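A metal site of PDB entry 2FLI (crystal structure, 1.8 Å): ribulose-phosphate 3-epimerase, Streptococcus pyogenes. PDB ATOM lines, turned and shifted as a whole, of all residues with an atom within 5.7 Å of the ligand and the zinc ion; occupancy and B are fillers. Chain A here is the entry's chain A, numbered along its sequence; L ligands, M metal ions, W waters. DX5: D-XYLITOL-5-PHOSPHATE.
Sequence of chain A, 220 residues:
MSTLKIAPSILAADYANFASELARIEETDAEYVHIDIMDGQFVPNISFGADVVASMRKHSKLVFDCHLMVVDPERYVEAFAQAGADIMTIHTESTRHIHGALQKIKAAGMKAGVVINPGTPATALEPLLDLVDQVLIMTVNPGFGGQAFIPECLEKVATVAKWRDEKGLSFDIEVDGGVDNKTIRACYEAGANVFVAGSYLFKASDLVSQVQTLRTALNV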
ATOM      1  N   SER A   9      10.183 -17.933 -12.744  1.00  0.00           N
ATOM      2  CA  SER A   9       9.096 -17.274 -12.029  1.00  0.00           C
ATOM      3  C   SER A   9       8.988 -15.804 -12.412  1.00  0.00           C
ATOM      4  O   SER A   9       9.853 -15.001 -12.074  1.00  0.00           O
ATOM      5  CB  SER A   9       9.305 -17.387 -10.520  1.00  0.00           C
ATOM      6  OG  SER A   9       8.199 -16.819  -9.842  1.00  0.00           O
ATOM      7  N   LEU A  11       7.401 -13.552 -11.217  1.00  0.00           N
ATOM      8  CA  LEU A  11       7.283 -12.651 -10.075  1.00  0.00           C
ATOM      9  C   LEU A  11       8.593 -11.898  -9.881  1.00  0.00           C
ATOM     10  O   LEU A  11       8.622 -10.839  -9.271  1.00  0.00           O
ATOM     11  CB  LEU A  11       6.965 -13.437  -8.805  1.00  0.00           C
ATOM     12  CG  LEU A  11       6.709 -12.636  -7.522  1.00  0.00           C
ATOM     13  CD1 LEU A  11       5.316 -12.011  -7.579  1.00  0.00           C
ATOM     14  CD2 LEU A  11       6.839 -13.545  -6.303  1.00  0.00           C
ATOM     15  N   ALA A  12       9.683 -12.467 -10.400  1.00  0.00           N
ATOM     16  CA  ALA A  12      11.002 -11.856 -10.261  1.00  0.00           C
ATOM     17  C   ALA A  12      11.385 -11.013 -11.476  1.00  0.00           C
ATOM     18  O   ALA A  12      12.501 -10.475 -11.540  1.00  0.00           O
ATOM     19  CB  ALA A  12      12.042 -12.950 -10.046  1.00  0.00           C
ATOM     20  N   HIS A  34       6.254 -19.763 -14.615  1.00  0.00           N
ATOM     21  CA  HIS A  34       5.592 -19.861 -13.327  1.00  0.00           C
ATOM     22  C   HIS A  34       4.956 -18.534 -12.927  1.00  0.00           C
ATOM     23  O   HIS A  34       5.666 -17.550 -12.696  1.00  0.00           O
ATOM     24  CB  HIS A  34       6.575 -20.282 -12.243  1.00  0.00           C
ATOM     25  CG  HIS A  34       5.922 -20.751 -10.998  1.00  0.00           C
ATOM     26  ND1 HIS A  34       5.318 -21.987 -10.890  1.00  0.00           N
ATOM     27  CD2 HIS A  34       5.728 -20.135  -9.809  1.00  0.00           C
ATOM     28  CE1 HIS A  34       4.787 -22.119  -9.685  1.00  0.00           C
ATOM     29  NE2 HIS A  34       5.022 -21.009  -9.012  1.00  0.00           N
ATOM     30  N   ILE A  35       3.635 -18.513 -12.835  1.00  0.00           N
ATOM     31  CA  ILE A  35       2.928 -17.285 -12.483  1.00  0.00           C
ATOM     32  C   ILE A  35       2.284 -17.327 -11.099  1.00  0.00           C
ATOM     33  O   ILE A  35       1.334 -18.073 -10.866  1.00  0.00           O
ATOM     34  CB  ILE A  35       1.865 -16.969 -13.534  1.00  0.00           C
ATOM     35  CG1 ILE A  35       2.498 -17.028 -14.925  1.00  0.00           C
ATOM     36  CG2 ILE A  35       1.271 -15.592 -13.276  1.00  0.00           C
ATOM     37  CD1 ILE A  35       1.523 -17.047 -16.077  1.00  0.00           C
ATOM     38  N   ASP A  36       2.828 -16.511 -10.198  1.00  0.00           N
ATOM     39  CA  ASP A  36       2.345 -16.436  -8.826  1.00  0.00           C
ATOM     40  C   ASP A  36       1.241 -15.402  -8.630  1.00  0.00           C
ATOM     41  O   ASP A  36       1.452 -14.203  -8.812  1.00  0.00           O
ATOM     42  CB  ASP A  36       3.504 -16.082  -7.892  1.00  0.00           C
ATOM     43  CG  ASP A  36       4.519 -17.181  -7.818  1.00  0.00           C
ATOM     44  OD1 ASP A  36       4.124 -18.284  -7.407  1.00  0.00           O
ATOM     45  OD2 ASP A  36       5.696 -16.954  -8.168  1.00  0.00           O
ATOM     46  N   MET A  38      -1.188 -13.656  -5.979  1.00  0.00           N
ATOM     47  CA  MET A  38      -1.287 -13.391  -4.544  1.00  0.00           C
ATOM     48  C   MET A  38      -2.385 -12.350  -4.296  1.00  0.00           C
ATOM     49  O   MET A  38      -2.433 -11.331  -4.984  1.00  0.00           O
ATOM     50  CB  MET A  38       0.057 -12.851  -4.017  1.00  0.00           C
ATOM     51  CG  MET A  38       1.217 -13.832  -4.101  1.00  0.00           C
ATOM     52  SD  MET A  38       2.779 -13.015  -3.669  1.00  0.00           S
ATOM     53  CE  MET A  38       3.969 -14.048  -4.486  1.00  0.00           C
ATOM     54  N   HIS A  67       0.128 -20.485 -10.060  1.00  0.00           N
ATOM     55  CA  HIS A  67       0.160 -20.863  -8.659  1.00  0.00           C
ATOM     56  C   HIS A  67      -0.695 -19.887  -7.864  1.00  0.00           C
ATOM     57  O   HIS A  67      -0.352 -18.715  -7.729  1.00  0.00           O
ATOM     58  CB  HIS A  67       1.624 -20.823  -8.197  1.00  0.00           C
ATOM     59  CG  HIS A  67       1.808 -21.123  -6.746  1.00  0.00           C
ATOM     60  ND1 HIS A  67       3.045 -21.052  -6.129  1.00  0.00           N
ATOM     61  CD2 HIS A  67       0.938 -21.472  -5.771  1.00  0.00           C
ATOM     62  CE1 HIS A  67       2.927 -21.348  -4.859  1.00  0.00           C
ATOM     63  NE2 HIS A  67       1.651 -21.612  -4.606  1.00  0.00           N
ATOM     64  N   MET A  69      -1.870 -18.283  -4.691  1.00  0.00           N
ATOM     65  CA  MET A  69      -1.666 -17.999  -3.284  1.00  0.00           C
ATOM     66  C   MET A  69      -2.771 -17.021  -2.897  1.00  0.00           C
ATOM     67  O   MET A  69      -2.518 -15.871  -2.539  1.00  0.00           O
ATOM     68  CB  MET A  69      -0.282 -17.397  -3.051  1.00  0.00           C
ATOM     69  CG  MET A  69       0.826 -18.414  -3.186  1.00  0.00           C
ATOM     70  SD  MET A  69       2.481 -17.702  -3.215  1.00  0.00           S
ATOM     71  CE  MET A  69       2.614 -17.341  -4.964  1.00  0.00           C
ATOM     72  N   LEU A 136       3.177 -29.732  -5.999  1.00  0.00           N
ATOM     73  CA  LEU A 136       4.196 -28.721  -5.745  1.00  0.00           C
ATOM     74  C   LEU A 136       4.556 -28.646  -4.272  1.00  0.00           C
ATOM     75  O   LEU A 136       3.689 -28.420  -3.420  1.00  0.00           O
ATOM     76  CB  LEU A 136       3.707 -27.349  -6.212  1.00  0.00           C
ATOM     77  CG  LEU A 136       4.472 -26.141  -5.667  1.00  0.00           C
ATOM     78  CD1 LEU A 136       5.959 -26.270  -5.990  1.00  0.00           C
ATOM     79  CD2 LEU A 136       3.907 -24.868  -6.278  1.00  0.00           C
ATOM     80  N   MET A 138       6.480 -26.488  -1.669  1.00  0.00           N
ATOM     81  CA  MET A 138       7.107 -25.182  -1.457  1.00  0.00           C
ATOM     82  C   MET A 138       8.401 -25.422  -0.693  1.00  0.00           C
ATOM     83  O   MET A 138       8.427 -26.221   0.254  1.00  0.00           O
ATOM     84  CB  MET A 138       6.225 -24.258  -0.603  1.00  0.00           C
ATOM     85  CG  MET A 138       4.952 -23.753  -1.283  1.00  0.00           C
ATOM     86  SD  MET A 138       5.280 -22.826  -2.789  1.00  0.00           S
ATOM     87  CE  MET A 138       6.567 -21.665  -2.246  1.00  0.00           C
ATOM     88  N   VAL A 140      10.136 -22.692   0.390  1.00  0.00           N
ATOM     89  CA  VAL A 140      10.247 -21.417   1.109  1.00  0.00           C
ATOM     90  C   VAL A 140       8.825 -21.100   1.495  1.00  0.00           C
ATOM     91  O   VAL A 140       7.896 -21.611   0.883  1.00  0.00           O
ATOM     92  CB  VAL A 140      10.766 -20.229   0.227  1.00  0.00           C
ATOM     93  CG1 VAL A 140      12.165 -20.538  -0.303  1.00  0.00           C
ATOM     94  CG2 VAL A 140       9.793 -19.926  -0.903  1.00  0.00           C
ATOM     95  N   ASN A 141       8.650 -20.266   2.525  1.00  0.00           N
ATOM     96  CA  ASN A 141       7.306 -19.891   2.939  1.00  0.00           C
ATOM     97  C   ASN A 141       6.779 -18.896   1.906  1.00  0.00           C
ATOM     98  O   ASN A 141       7.374 -17.838   1.678  1.00  0.00           O
ATOM     99  CB  ASN A 141       7.333 -19.275   4.342  1.00  0.00           C
ATOM    100  CG  ASN A 141       7.556 -20.316   5.416  1.00  0.00           C
ATOM    101  OD1 ASN A 141       6.656 -21.103   5.720  1.00  0.00           O
ATOM    102  ND2 ASN A 141       8.755 -20.347   5.993  1.00  0.00           N
ATOM    103  N   PRO A 142       5.651 -19.228   1.260  1.00  0.00           N
ATOM    104  CA  PRO A 142       4.998 -18.410   0.220  1.00  0.00           C
ATOM    105  C   PRO A 142       4.910 -16.922   0.543  1.00  0.00           C
ATOM    106  O   PRO A 142       4.666 -16.545   1.679  1.00  0.00           O
ATOM    107  CB  PRO A 142       3.615 -19.043   0.109  1.00  0.00           C
ATOM    108  CG  PRO A 142       3.866 -20.463   0.451  1.00  0.00           C
ATOM    109  CD  PRO A 142       4.781 -20.356   1.639  1.00  0.00           C
ATOM    110  N   GLY A 143       5.104 -16.089  -0.475  1.00  0.00           N
ATOM    111  CA  GLY A 143       4.998 -14.657  -0.248  1.00  0.00           C
ATOM    112  C   GLY A 143       5.914 -13.776  -1.066  1.00  0.00           C
ATOM    113  O   GLY A 143       5.493 -12.721  -1.541  1.00  0.00           O
ATOM    114  N   PHE A 144       7.156 -14.197  -1.238  1.00  0.00           N
ATOM    115  CA  PHE A 144       8.115 -13.393  -2.002  1.00  0.00           C
ATOM    116  C   PHE A 144       9.375 -14.166  -2.363  1.00  0.00           C
ATOM    117  O   PHE A 144       9.661 -15.215  -1.802  1.00  0.00           O
ATOM    118  CB  PHE A 144       8.463 -12.118  -1.229  1.00  0.00           C
ATOM    119  CG  PHE A 144       8.703 -12.346   0.225  1.00  0.00           C
ATOM    120  CD1 PHE A 144       9.969 -12.679   0.707  1.00  0.00           C
ATOM    121  CD2 PHE A 144       7.649 -12.240   1.143  1.00  0.00           C
ATOM    122  CE1 PHE A 144      10.182 -12.910   2.074  1.00  0.00           C
ATOM    123  CE2 PHE A 144       7.842 -12.470   2.497  1.00  0.00           C
ATOM    124  CZ  PHE A 144       9.121 -12.805   2.974  1.00  0.00           C
ATOM    125  N   GLY A 145      10.127 -13.631  -3.330  1.00  0.00           N
ATOM    126  CA  GLY A 145      11.339 -14.292  -3.759  1.00  0.00           C
ATOM    127  C   GLY A 145      12.551 -13.975  -2.908  1.00  0.00           C
ATOM    128  O   GLY A 145      12.437 -13.278  -1.900  1.00  0.00           O
ATOM    129  N   GLY A 146      13.702 -14.500  -3.315  1.00  0.00           N
ATOM    130  CA  GLY A 146      14.943 -14.248  -2.609  1.00  0.00           C
ATOM    131  C   GLY A 146      15.050 -14.887  -1.224  1.00  0.00           C
ATOM    132  O   GLY A 146      16.052 -14.688  -0.546  1.00  0.00           O
ATOM    133  N   GLN A 147      14.048 -15.648  -0.816  1.00  0.00           N
ATOM    134  CA  GLN A 147      14.077 -16.301   0.495  1.00  0.00           C
ATOM    135  C   GLN A 147      15.052 -17.461   0.559  1.00  0.00           C
ATOM    136  O   GLN A 147      15.458 -18.004  -0.464  1.00  0.00           O
ATOM    137  CB  GLN A 147      12.678 -16.799   0.887  1.00  0.00           C
ATOM    138  CG  GLN A 147      11.693 -15.694   1.190  1.00  0.00           C
ATOM    139  CD  GLN A 147      10.350 -16.236   1.629  1.00  0.00           C
ATOM    140  OE1 GLN A 147       9.493 -16.555   0.796  1.00  0.00           O
ATOM    141  NE2 GLN A 147      10.161 -16.356   2.933  1.00  0.00           N
ATOM    142  N   ASP A 176       9.470 -25.093  -5.369  1.00  0.00           N
ATOM    143  CA  ASP A 176       9.417 -23.663  -5.586  1.00  0.00           C
ATOM    144  C   ASP A 176       9.882 -22.865  -4.380  1.00  0.00           C
ATOM    145  O   ASP A 176       9.272 -22.919  -3.302  1.00  0.00           O
ATOM    146  CB  ASP A 176       7.993 -23.281  -5.965  1.00  0.00           C
ATOM    147  CG  ASP A 176       7.838 -21.823  -6.241  1.00  0.00           C
ATOM    148  OD1 ASP A 176       8.825 -21.162  -6.611  1.00  0.00           O
ATOM    149  OD2 ASP A 176       6.703 -21.329  -6.098  1.00  0.00           O
ATOM    150  N   GLY A 177      10.982 -22.139  -4.553  1.00  0.00           N
ATOM    151  CA  GLY A 177      11.522 -21.331  -3.476  1.00  0.00           C
ATOM    152  C   GLY A 177      12.984 -21.585  -3.212  1.00  0.00           C
ATOM    153  O   GLY A 177      13.375 -22.694  -2.828  1.00  0.00           O
ATOM    154  N   GLY A 178      13.809 -20.571  -3.442  1.00  0.00           N
ATOM    155  CA  GLY A 178      15.231 -20.714  -3.206  1.00  0.00           C
ATOM    156  C   GLY A 178      15.920 -21.762  -4.067  1.00  0.00           C
ATOM    157  O   GLY A 178      16.967 -22.279  -3.684  1.00  0.00           O
ATOM    158  N   VAL A 179      15.348 -22.085  -5.222  1.00  0.00           N
ATOM    159  CA  VAL A 179      15.973 -23.048  -6.120  1.00  0.00           C
ATOM    160  C   VAL A 179      17.012 -22.322  -6.973  1.00  0.00           C
ATOM    161  O   VAL A 179      16.675 -21.406  -7.728  1.00  0.00           O
ATOM    162  CB  VAL A 179      14.946 -23.709  -7.078  1.00  0.00           C
ATOM    163  CG1 VAL A 179      15.666 -24.705  -7.989  1.00  0.00           C
ATOM    164  CG2 VAL A 179      13.874 -24.424  -6.277  1.00  0.00           C
ATOM    165  N   VAL A 196      11.014 -24.422 -10.197  1.00  0.00           N
ATOM    166  CA  VAL A 196      10.680 -23.010 -10.309  1.00  0.00           C
ATOM    167  C   VAL A 196      11.820 -22.176  -9.739  1.00  0.00           C
ATOM    168  O   VAL A 196      12.326 -22.472  -8.658  1.00  0.00           O
ATOM    169  CB  VAL A 196       9.399 -22.679  -9.526  1.00  0.00           C
ATOM    170  CG1 VAL A 196       9.075 -21.184  -9.660  1.00  0.00           C
ATOM    171  CG2 VAL A 196       8.235 -23.523 -10.052  1.00  0.00           C
ATOM    172  N   ALA A 197      12.226 -21.144 -10.483  1.00  0.00           N
ATOM    173  CA  ALA A 197      13.318 -20.269 -10.061  1.00  0.00           C
ATOM    174  C   ALA A 197      12.997 -18.819 -10.420  1.00  0.00           C
ATOM    175  O   ALA A 197      12.708 -18.504 -11.570  1.00  0.00           O
ATOM    176  CB  ALA A 197      14.604 -20.689 -10.718  1.00  0.00           C
ATOM    177  N   GLY A 198      13.071 -17.937  -9.431  1.00  0.00           N
ATOM    178  CA  GLY A 198      12.785 -16.545  -9.669  1.00  0.00           C
ATOM    179  C   GLY A 198      14.034 -15.679  -9.678  1.00  0.00           C
ATOM    180  O   GLY A 198      14.653 -15.468 -10.721  1.00  0.00           O
ATOM    181  N   SER A 199      14.402 -15.177  -8.511  1.00  0.00           N
ATOM    182  CA  SER A 199      15.566 -14.293  -8.368  1.00  0.00           C
ATOM    183  C   SER A 199      16.876 -14.803  -8.972  1.00  0.00           C
ATOM    184  O   SER A 199      17.652 -14.021  -9.517  1.00  0.00           O
ATOM    185  CB  SER A 199      15.777 -13.955  -6.893  1.00  0.00           C
ATOM    186  OG  SER A 199      16.018 -15.125  -6.139  1.00  0.00           O
ATOM    187  N   TYR A 200      17.140 -16.103  -8.864  1.00  0.00           N
ATOM    188  CA  TYR A 200      18.383 -16.643  -9.405  1.00  0.00           C
ATOM    189  C   TYR A 200      18.490 -16.457 -10.920  1.00  0.00           C
ATOM    190  O   TYR A 200      19.578 -16.268 -11.458  1.00  0.00           O
ATOM    191  CB  TYR A 200      18.540 -18.122  -9.073  1.00  0.00           C
ATOM    192  CG  TYR A 200      19.770 -18.729  -9.689  1.00  0.00           C
ATOM    193  CD1 TYR A 200      21.036 -18.414  -9.195  1.00  0.00           C
ATOM    194  CD2 TYR A 200      19.691 -19.584 -10.787  1.00  0.00           C
ATOM    195  CE1 TYR A 200      22.187 -18.932  -9.787  1.00  0.00           C
ATOM    196  CE2 TYR A 200      20.825 -20.101 -11.383  1.00  0.00           C
ATOM    197  CZ  TYR A 200      22.071 -19.765 -10.872  1.00  0.00           C
ATOM    198  OH  TYR A 200      23.207 -20.268 -11.470  1.00  0.00           O
HETATM  199  C1  DX5 L   1       7.022 -17.541  -3.554  1.00  0.00           C
HETATM  200  C2  DX5 L   1       6.724 -17.733  -5.019  1.00  0.00           C
HETATM  201  C3  DX5 L   1       7.893 -18.230  -5.815  1.00  0.00           C
HETATM  202  C4  DX5 L   1       8.963 -17.207  -6.016  1.00  0.00           C
HETATM  203  C5  DX5 L   1      10.340 -17.790  -6.206  1.00  0.00           C
HETATM  204  O1  DX5 L   1       5.895 -17.068  -2.816  1.00  0.00           O
HETATM  205  O2  DX5 L   1       5.611 -18.639  -5.115  1.00  0.00           O
HETATM  206  O3  DX5 L   1       7.481 -18.752  -7.103  1.00  0.00           O
HETATM  207  O4  DX5 L   1       8.716 -16.384  -7.168  1.00  0.00           O
HETATM  208  O5  DX5 L   1      11.497 -17.032  -5.907  1.00  0.00           O
HETATM  209  P   DX5 L   1      12.897 -17.474  -5.697  1.00  0.00           P
HETATM  210  O1P DX5 L   1      13.238 -18.480  -6.864  1.00  0.00           O
HETATM  211  O2P DX5 L   1      12.859 -18.118  -4.262  1.00  0.00           O
HETATM  212  O3P DX5 L   1      13.713 -16.080  -5.788  1.00  0.00           O
HETATM  213 ZN    ZN M   1       4.914 -20.244  -7.004  1.00  0.00          ZN
HETATM  214  O   HOH W   1      11.467 -17.077  -2.171  1.00  0.00           O
HETATM  215  O   HOH W   2      12.819 -21.086  -6.534  1.00  0.00           O
HETATM  216  O   HOH W   3      10.815 -14.754  -7.318  1.00  0.00           O
HETATM  217  O   HOH W   4      15.248 -17.455  -3.166  1.00  0.00           O
HETATM  218  O   HOH W   5      15.813 -18.832  -7.631  1.00  0.00           O
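The backbone NH of Ser 199 is in hydrogen-bond range of an oxygen (O3P) of the ligand. The side-chain hydroxyl (OG) of Ser 199 lies within hydrogen-bond range of an oxygen (O3P) of the ligand. The backbone NH (N) of Gly 198 sits at hydrogen-bond distance from an oxygen (O1P) of the ligand, 2.6 Å away. N of Gly 143 lies within hydrogen-bond range of O1 of the ligand (2.7 Å). O2P of the ligand is in hydrogen-bond range of N of Gly 178 (2.8 Å). OG of Ser 9 is in hydrogen-bond range of O4 of the ligand. The backbone NH (N) of Gly 146 sits at hydrogen-bond distance from an oxygen (O3P) of the ligand (2.9 Å). An oxygen (O1) of the ligand sits at hydrogen-bond distance from the side-chain sulfur (SD) of Met 69, 3.5 Å away.
OD2 of Asp 36 lies within hydrogen-bond range of OG of Ser 9 (3.0 Å). The backbone carbonyl oxygen of Ile 35 is in hydrogen-bond range of the backbone NH of His 67. O of Ala 197 lies within hydrogen-bond range of N of Ser 9, at 2.8 Å. The backbone carbonyl oxygen (O) of Phe 144 lies close to the side-chain amide oxygen (OE1) of Gln 147, 2.9 Å away.
Residues that only touch the ligand: Leu 11 (3.5 Å), Met 38 (3.95 Å), Pro 142 (3.4 Å), Phe 144 (3.5 Å), Gly 145 (3.5 Å), Gly 177 (3.6 Å), Val 196 (3.9 Å) and Ala 197 (3.6 Å). Hydrophobic or aromatic side chains within 4 Å of the ligand: Leu 11, His 34, Met 38, His 67, Met 69 and Val 196. The nearest printed residue that does not touch the ligand is Met 138 (4.3 Å).
Four residues have an atom within 4 Å of the zinc ion: His 34, Asp 36, His 67 and Asp 176. The nearest printed residue that does not touch the zinc ion is Met 69 (4.2 Å).
The zinc ion is bound by OD1 of Asp 36 (2.2 Å). NE2 of His 34 binds the zinc ion. The zinc ion is bound by ND1 of His 67, 2.2 Å away. The side-chain carboxylate (OD2) of Asp 176 is bound to the zinc ion. The zinc ion is bound by an oxygen (O2) of the ligand (2.6 Å). The zinc ion has five donor atoms within binding distance.
Water W5 lies within hydrogen-bond range of an oxygen (O1P) of the ligand (2.7 Å), the backbone carbonyl oxygen (O) of Val 179 (2.7 Å), the backbone NH (N) of Tyr 200 (3.3 Å) and the backbone NH (N) of Gly 198 (3.4 Å). Water W4 lies within hydrogen-bond range of an oxygen (O2P) of the ligand (2.7 Å), the backbone carbonyl oxygen of Gln 147 (2.8 Å), the backbone NH of Gly 146 (3.3 Å) and the backbone NH of Gly 178 (3.4 Å). Water W1 lies within hydrogen-bond range of the backbone carbonyl oxygen of Phe 144 (2.6 Å), an oxygen (O2P) of the ligand (2.7 Å) and the backbone NH of Gln 147 (3.2 Å).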
